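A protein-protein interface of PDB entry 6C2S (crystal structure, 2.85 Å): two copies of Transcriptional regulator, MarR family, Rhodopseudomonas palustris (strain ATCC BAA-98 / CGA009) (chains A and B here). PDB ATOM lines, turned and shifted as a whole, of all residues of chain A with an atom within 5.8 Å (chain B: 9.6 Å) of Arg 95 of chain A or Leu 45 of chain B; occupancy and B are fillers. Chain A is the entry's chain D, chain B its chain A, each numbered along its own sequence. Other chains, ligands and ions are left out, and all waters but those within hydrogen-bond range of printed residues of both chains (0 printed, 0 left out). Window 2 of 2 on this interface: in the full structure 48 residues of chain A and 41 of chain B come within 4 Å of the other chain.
Among the printed residues, merely in contact across the chains: Leu 88 of chain A with Lys 46 of chain B, Asn 92 of chain A with Leu 45 of chain B, Arg 95 of chain A with Leu 45 of chain B, Glu 99 of chain A with Leu 45 of chain B and Ile 100 of chain A with Leu 45 of chain B.
ND2 of Asn 92 of chain A lies within hydrogen-bond range of O of Lys 46 of chain B.
No position is printed for both chains.
Of the 8 printed residues of chain B, 2 touch a printed residue of chain A. Hydrophobic or aromatic side chains of chain B within 4 Å of the printed part of chain A: Leu 45. Of the 13 printed residues of chain A, 5 touch a printed residue of chain B. Among the printed residues, 6 pairs touch across the chains.
The backbone carbonyl oxygen of Arg 95 of chain A is in hydrogen-bond range of the backbone NH of Leu 138 of chain A, at 3.0 Å. The backbone carbonyl oxygen (O) of Leu 88 of chain A lies within hydrogen-bond range of the side-chain amide nitrogen (ND2) of Asn 92 of chain A. NH1 of Arg 95 of chain A lies within salt-bridge range of OE2 of Glu 99 of chain A (2.9 Å). The side-chain amide oxygen of Asn 96 of chain A lies close to the side-chain carboxylate of Glu 99 of chain A, at 2.9 Å.
Printed residues of chain B within 4 Å of Leu 88 of chain A: Lys 46. Of the printed residues of chain B, Asn 92 of chain A touches Leu 45 and Lys 46. No residue of chain B comes within 4 Å of Gly 94 of chain A. Printed residues of chain B within 4 Å of Arg 95 of chain A: Leu 45. Printed residues of chain B within 4 Å of Glu 99 of chain A: Leu 45. Of the printed residues of chain B, Ile 100 of chain A touches Leu 45 (3.8 Å). No residue of chain B comes within 4 Å of Leu 138 of chain A. Leu 45 of chain B touches just these residues of chain A: Asn 92, Arg 95, Glu 99 and Ile 100. The nearest printed residue of chain B that does not touch Arg 95 of chain A is Glu 44 of chain B (4.002 Å). The nearest residue of chain A that does not touch Leu 45 of chain B is Thr 103 of chain A (4.2 Å).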
ATOM      1  N   LEU A  88      -2.715 -16.887 -14.860  1.00  0.00           N
ATOM      2  CA  LEU A  88      -1.602 -16.580 -13.976  1.00  0.00           C
ATOM      3  C   LEU A  88      -2.004 -16.744 -12.513  1.00  0.00           C
ATOM      4  O   LEU A  88      -1.205 -17.170 -11.683  1.00  0.00           O
ATOM      5  CB  LEU A  88      -1.135 -15.170 -14.267  1.00  0.00           C
ATOM      6  CG  LEU A  88       0.243 -14.716 -13.856  1.00  0.00           C
ATOM      7  CD1 LEU A  88       1.185 -15.779 -14.307  1.00  0.00           C
ATOM      8  CD2 LEU A  88       0.467 -13.499 -14.665  1.00  0.00           C
ATOM      9  N   ASN A  92      -0.128 -18.907  -9.832  1.00  0.00           N
ATOM     10  CA  ASN A  92       0.447 -18.122  -8.731  1.00  0.00           C
ATOM     11  C   ASN A  92      -0.641 -17.683  -7.748  1.00  0.00           C
ATOM     12  O   ASN A  92      -1.047 -16.510  -7.721  1.00  0.00           O
ATOM     13  CB  ASN A  92       1.214 -16.907  -9.260  1.00  0.00           C
ATOM     14  CG  ASN A  92       2.327 -17.292 -10.211  1.00  0.00           C
ATOM     15  OD1 ASN A  92       3.468 -17.491  -9.807  1.00  0.00           O
ATOM     16  ND2 ASN A  92       1.993 -17.413 -11.489  1.00  0.00           N
ATOM     17  N   PRO A  93      -1.129 -18.604  -6.924  1.00  0.00           N
ATOM     18  CA  PRO A  93      -2.068 -18.234  -5.859  1.00  0.00           C
ATOM     19  C   PRO A  93      -1.356 -17.532  -4.710  1.00  0.00           C
ATOM     20  O   PRO A  93      -0.135 -17.628  -4.549  1.00  0.00           O
ATOM     21  CB  PRO A  93      -2.635 -19.584  -5.416  1.00  0.00           C
ATOM     22  CG  PRO A  93      -1.494 -20.548  -5.665  1.00  0.00           C
ATOM     23  CD  PRO A  93      -0.632 -19.982  -6.772  1.00  0.00           C
ATOM     24  N   GLY A  94      -2.135 -16.781  -3.923  1.00  0.00           N
ATOM     25  CA  GLY A  94      -1.565 -16.116  -2.768  1.00  0.00           C
ATOM     26  C   GLY A  94      -0.925 -14.772  -3.039  1.00  0.00           C
ATOM     27  O   GLY A  94      -0.404 -14.150  -2.103  1.00  0.00           O
ATOM     28  N   ARG A  95      -0.912 -14.321  -4.283  1.00  0.00           N
ATOM     29  CA  ARG A  95      -0.303 -13.058  -4.653  1.00  0.00           C
ATOM     30  C   ARG A  95      -1.279 -11.892  -4.415  1.00  0.00           C
ATOM     31  O   ARG A  95      -2.417 -12.077  -3.978  1.00  0.00           O
ATOM     32  CB  ARG A  95       0.141 -13.130  -6.106  1.00  0.00           C
ATOM     33  CG  ARG A  95       1.284 -14.090  -6.324  1.00  0.00           C
ATOM     34  CD  ARG A  95       2.411 -13.848  -5.346  1.00  0.00           C
ATOM     35  NE  ARG A  95       3.625 -14.563  -5.726  1.00  0.00           N
ATOM     36  CZ  ARG A  95       4.840 -14.251  -5.289  1.00  0.00           C
ATOM     37  NH1 ARG A  95       4.999 -13.235  -4.452  1.00  0.00           N
ATOM     38  NH2 ARG A  95       5.895 -14.949  -5.693  1.00  0.00           N
ATOM     39  N   ASN A  96      -0.780 -10.670  -4.565  1.00  0.00           N
ATOM     40  CA  ASN A  96      -1.612  -9.481  -4.456  1.00  0.00           C
ATOM     41  C   ASN A  96      -1.766  -8.809  -5.833  1.00  0.00           C
ATOM     42  O   ASN A  96      -1.229  -9.267  -6.850  1.00  0.00           O
ATOM     43  CB  ASN A  96      -1.068  -8.528  -3.384  1.00  0.00           C
ATOM     44  CG  ASN A  96       0.170  -7.765  -3.832  1.00  0.00           C
ATOM     45  OD1 ASN A  96       0.870  -8.176  -4.766  1.00  0.00           O
ATOM     46  ND2 ASN A  96       0.466  -6.659  -3.139  1.00  0.00           N
ATOM     47  N   GLN A  97      -2.545  -7.722  -5.873  1.00  0.00           N
ATOM     48  CA  GLN A  97      -2.797  -7.053  -7.143  1.00  0.00           C
ATOM     49  C   GLN A  97      -1.510  -6.543  -7.775  1.00  0.00           C
ATOM     50  O   GLN A  97      -1.206  -6.859  -8.929  1.00  0.00           O
ATOM     51  CB  GLN A  97      -3.786  -5.918  -6.940  1.00  0.00           C
ATOM     52  CG  GLN A  97      -5.151  -6.411  -6.587  1.00  0.00           C
ATOM     53  CD  GLN A  97      -6.120  -5.279  -6.437  1.00  0.00           C
ATOM     54  OE1 GLN A  97      -7.117  -5.391  -5.728  1.00  0.00           O
ATOM     55  NE2 GLN A  97      -5.800  -4.151  -7.054  1.00  0.00           N
ATOM     56  N   GLU A  99       1.441  -7.446  -7.668  1.00  0.00           N
ATOM     57  CA  GLU A  99       2.275  -8.525  -8.209  1.00  0.00           C
ATOM     58  C   GLU A  99       1.672  -9.130  -9.473  1.00  0.00           C
ATOM     59  O   GLU A  99       2.383  -9.368 -10.458  1.00  0.00           O
ATOM     60  CB  GLU A  99       2.481  -9.608  -7.149  1.00  0.00           C
ATOM     61  CG  GLU A  99       3.460  -9.268  -6.047  1.00  0.00           C
ATOM     62  CD  GLU A  99       3.342 -10.220  -4.862  1.00  0.00           C
ATOM     63  OE1 GLU A  99       2.236 -10.767  -4.666  1.00  0.00           O
ATOM     64  OE2 GLU A  99       4.344 -10.433  -4.138  1.00  0.00           O
ATOM     65  N   ILE A 100       0.375  -9.446  -9.443  1.00  0.00           N
ATOM     66  CA  ILE A 100      -0.290  -9.964 -10.639  1.00  0.00           C
ATOM     67  C   ILE A 100      -0.288  -8.917 -11.747  1.00  0.00           C
ATOM     68  O   ILE A 100       0.034  -9.214 -12.899  1.00  0.00           O
ATOM     69  CB  ILE A 100      -1.716 -10.446 -10.316  1.00  0.00           C
ATOM     70  CG1 ILE A 100      -1.665 -11.588  -9.308  1.00  0.00           C
ATOM     71  CG2 ILE A 100      -2.380 -10.945 -11.568  1.00  0.00           C
ATOM     72  CD1 ILE A 100      -0.945 -12.804  -9.847  1.00  0.00           C
ATOM     73  N   THR A 103       3.238  -8.138 -13.487  1.00  0.00           N
ATOM     74  CA  THR A 103       3.760  -9.243 -14.279  1.00  0.00           C
ATOM     75  C   THR A 103       3.097  -9.304 -15.650  1.00  0.00           C
ATOM     76  O   THR A 103       3.670  -9.854 -16.600  1.00  0.00           O
ATOM     77  CB  THR A 103       3.626 -10.556 -13.488  1.00  0.00           C
ATOM     78  OG1 THR A 103       4.538 -11.532 -14.007  1.00  0.00           O
ATOM     79  CG2 THR A 103       2.240 -11.094 -13.544  1.00  0.00           C
ATOM     80  N   HIS A 136      -4.257  -7.069  -1.015  1.00  0.00           N
ATOM     81  CA  HIS A 136      -5.413  -7.882  -1.362  1.00  0.00           C
ATOM     82  C   HIS A 136      -4.868  -9.167  -1.942  1.00  0.00           C
ATOM     83  O   HIS A 136      -4.175  -9.138  -2.957  1.00  0.00           O
ATOM     84  CB  HIS A 136      -6.310  -7.170  -2.368  1.00  0.00           C
ATOM     85  CG  HIS A 136      -7.140  -6.095  -1.760  1.00  0.00           C
ATOM     86  ND1 HIS A 136      -7.912  -5.239  -2.510  1.00  0.00           N
ATOM     87  CD2 HIS A 136      -7.290  -5.709  -0.471  1.00  0.00           C
ATOM     88  CE1 HIS A 136      -8.527  -4.387  -1.708  1.00  0.00           C
ATOM     89  NE2 HIS A 136      -8.164  -4.649  -0.465  1.00  0.00           N
ATOM     90  N   ILE A 137      -5.094 -10.250  -1.288  1.00  0.00           N
ATOM     91  CA  ILE A 137      -4.669 -11.528  -1.837  1.00  0.00           C
ATOM     92  C   ILE A 137      -5.760 -12.106  -2.734  1.00  0.00           C
ATOM     93  O   ILE A 137      -6.952 -12.084  -2.394  1.00  0.00           O
ATOM     94  CB  ILE A 137      -4.257 -12.481  -0.705  1.00  0.00           C
ATOM     95  CG1 ILE A 137      -3.397 -11.710   0.315  1.00  0.00           C
ATOM     96  CG2 ILE A 137      -3.519 -13.647  -1.286  1.00  0.00           C
ATOM     97  CD1 ILE A 137      -1.930 -11.548  -0.081  1.00  0.00           C
ATOM     98  N   LEU A 138      -5.337 -12.627  -3.893  1.00  0.00           N
ATOM     99  CA  LEU A 138      -6.222 -13.055  -4.978  1.00  0.00           C
ATOM    100  C   LEU A 138      -6.054 -14.539  -5.257  1.00  0.00           C
ATOM    101  O   LEU A 138      -4.931 -15.007  -5.478  1.00  0.00           O
ATOM    102  CB  LEU A 138      -5.931 -12.270  -6.258  1.00  0.00           C
ATOM    103  CG  LEU A 138      -5.749 -10.770  -6.064  1.00  0.00           C
ATOM    104  CD1 LEU A 138      -5.247 -10.059  -7.303  1.00  0.00           C
ATOM    105  CD2 LEU A 138      -7.066 -10.163  -5.585  1.00  0.00           C
ATOM    106  N   SER B  43       9.871 -15.213  -4.855  1.00  0.00           N
ATOM    107  CA  SER B  43       9.716 -13.768  -5.041  1.00  0.00           C
ATOM    108  C   SER B  43       9.590 -13.373  -6.534  1.00  0.00           C
ATOM    109  O   SER B  43       9.432 -12.193  -6.847  1.00  0.00           O
ATOM    110  CB  SER B  43      10.855 -13.006  -4.360  1.00  0.00           C
ATOM    111  N   GLU B  44       9.751 -14.328  -7.457  1.00  0.00           N
ATOM    112  CA  GLU B  44       9.391 -14.114  -8.857  1.00  0.00           C
ATOM    113  C   GLU B  44       8.227 -15.034  -9.216  1.00  0.00           C
ATOM    114  O   GLU B  44       8.169 -16.177  -8.748  1.00  0.00           O
ATOM    115  CB  GLU B  44      10.586 -14.370  -9.791  1.00  0.00           C
ATOM    116  N   LEU B  45       7.292 -14.537 -10.039  1.00  0.00           N
ATOM    117  CA  LEU B  45       6.057 -15.278 -10.306  1.00  0.00           C
ATOM    118  C   LEU B  45       6.236 -16.267 -11.457  1.00  0.00           C
ATOM    119  O   LEU B  45       6.995 -16.021 -12.403  1.00  0.00           O
ATOM    120  CB  LEU B  45       4.874 -14.351 -10.615  1.00  0.00           C
ATOM    121  CG  LEU B  45       4.374 -13.320  -9.590  1.00  0.00           C
ATOM    122  CD1 LEU B  45       5.058 -11.948  -9.796  1.00  0.00           C
ATOM    123  CD2 LEU B  45       2.854 -13.223  -9.501  1.00  0.00           C
ATOM    124  N   LYS B  46       5.513 -17.394 -11.372  1.00  0.00           N
ATOM    125  CA  LYS B  46       5.564 -18.433 -12.396  1.00  0.00           C
ATOM    126  C   LYS B  46       4.671 -18.062 -13.573  1.00  0.00           C
ATOM    127  O   LYS B  46       3.479 -17.773 -13.402  1.00  0.00           O
ATOM    128  CB  LYS B  46       5.139 -19.802 -11.841  1.00  0.00           C
ATOM    129  CG  LYS B  46       6.243 -20.584 -11.105  1.00  0.00           C
ATOM    130  CD  LYS B  46       5.735 -21.799 -10.313  1.00  0.00           C
ATOM    131  CE  LYS B  46       6.930 -22.651  -9.834  1.00  0.00           C
ATOM    132  NZ  LYS B  46       6.637 -23.635  -8.730  1.00  0.00           N
ATOM    133  N   MET B  47       5.237 -18.077 -14.774  1.00  0.00           N
ATOM    134  CA  MET B  47       4.448 -17.619 -15.904  1.00  0.00           C
ATOM    135  C   MET B  47       3.482 -18.684 -16.401  1.00  0.00           C
ATOM    136  O   MET B  47       2.719 -18.426 -17.336  1.00  0.00           O
ATOM    137  CB  MET B  47       5.362 -17.142 -17.024  1.00  0.00           C
ATOM    138  CG  MET B  47       5.878 -15.757 -16.687  1.00  0.00           C
ATOM    139  SD  MET B  47       4.970 -14.418 -17.457  1.00  0.00           S
ATOM    140  CE  MET B  47       4.963 -14.941 -19.176  1.00  0.00           C
ATOM    141  N   GLY B  48       3.484 -19.857 -15.779  1.00  0.00           N
ATOM    142  CA  GLY B  48       2.477 -20.864 -16.045  1.00  0.00           C
ATOM    143  C   GLY B  48       2.379 -21.213 -17.508  1.00  0.00           C
ATOM    144  O   GLY B  48       3.389 -21.304 -18.225  1.00  0.00           O
ATOM    145  N   LEU B  50       1.155 -19.388 -19.774  1.00  0.00           N
ATOM    146  CA  LEU B  50       1.265 -18.210 -20.628  1.00  0.00           C
ATOM    147  C   LEU B  50       2.460 -18.297 -21.554  1.00  0.00           C
ATOM    148  O   LEU B  50       2.436 -17.733 -22.649  1.00  0.00           O
ATOM    149  CB  LEU B  50       1.382 -16.949 -19.789  1.00  0.00           C
ATOM    150  CG  LEU B  50       0.163 -16.063 -19.627  1.00  0.00           C
ATOM    151  CD1 LEU B  50      -0.914 -16.812 -18.902  1.00  0.00           C
ATOM    152  CD2 LEU B  50       0.581 -14.829 -18.848  1.00  0.00           C
ATOM    153  N   SER B  51       3.521 -18.962 -21.121  1.00  0.00           N
ATOM    154  CA  SER B  51       4.702 -19.095 -21.958  1.00  0.00           C
ATOM    155  C   SER B  51       4.403 -19.783 -23.285  1.00  0.00           C
ATOM    156  O   SER B  51       5.151 -19.584 -24.248  1.00  0.00           O
ATOM    157  CB  SER B  51       5.772 -19.878 -21.201  1.00  0.00           C
ATOM    158  OG  SER B  51       5.873 -19.414 -19.866  1.00  0.00           O
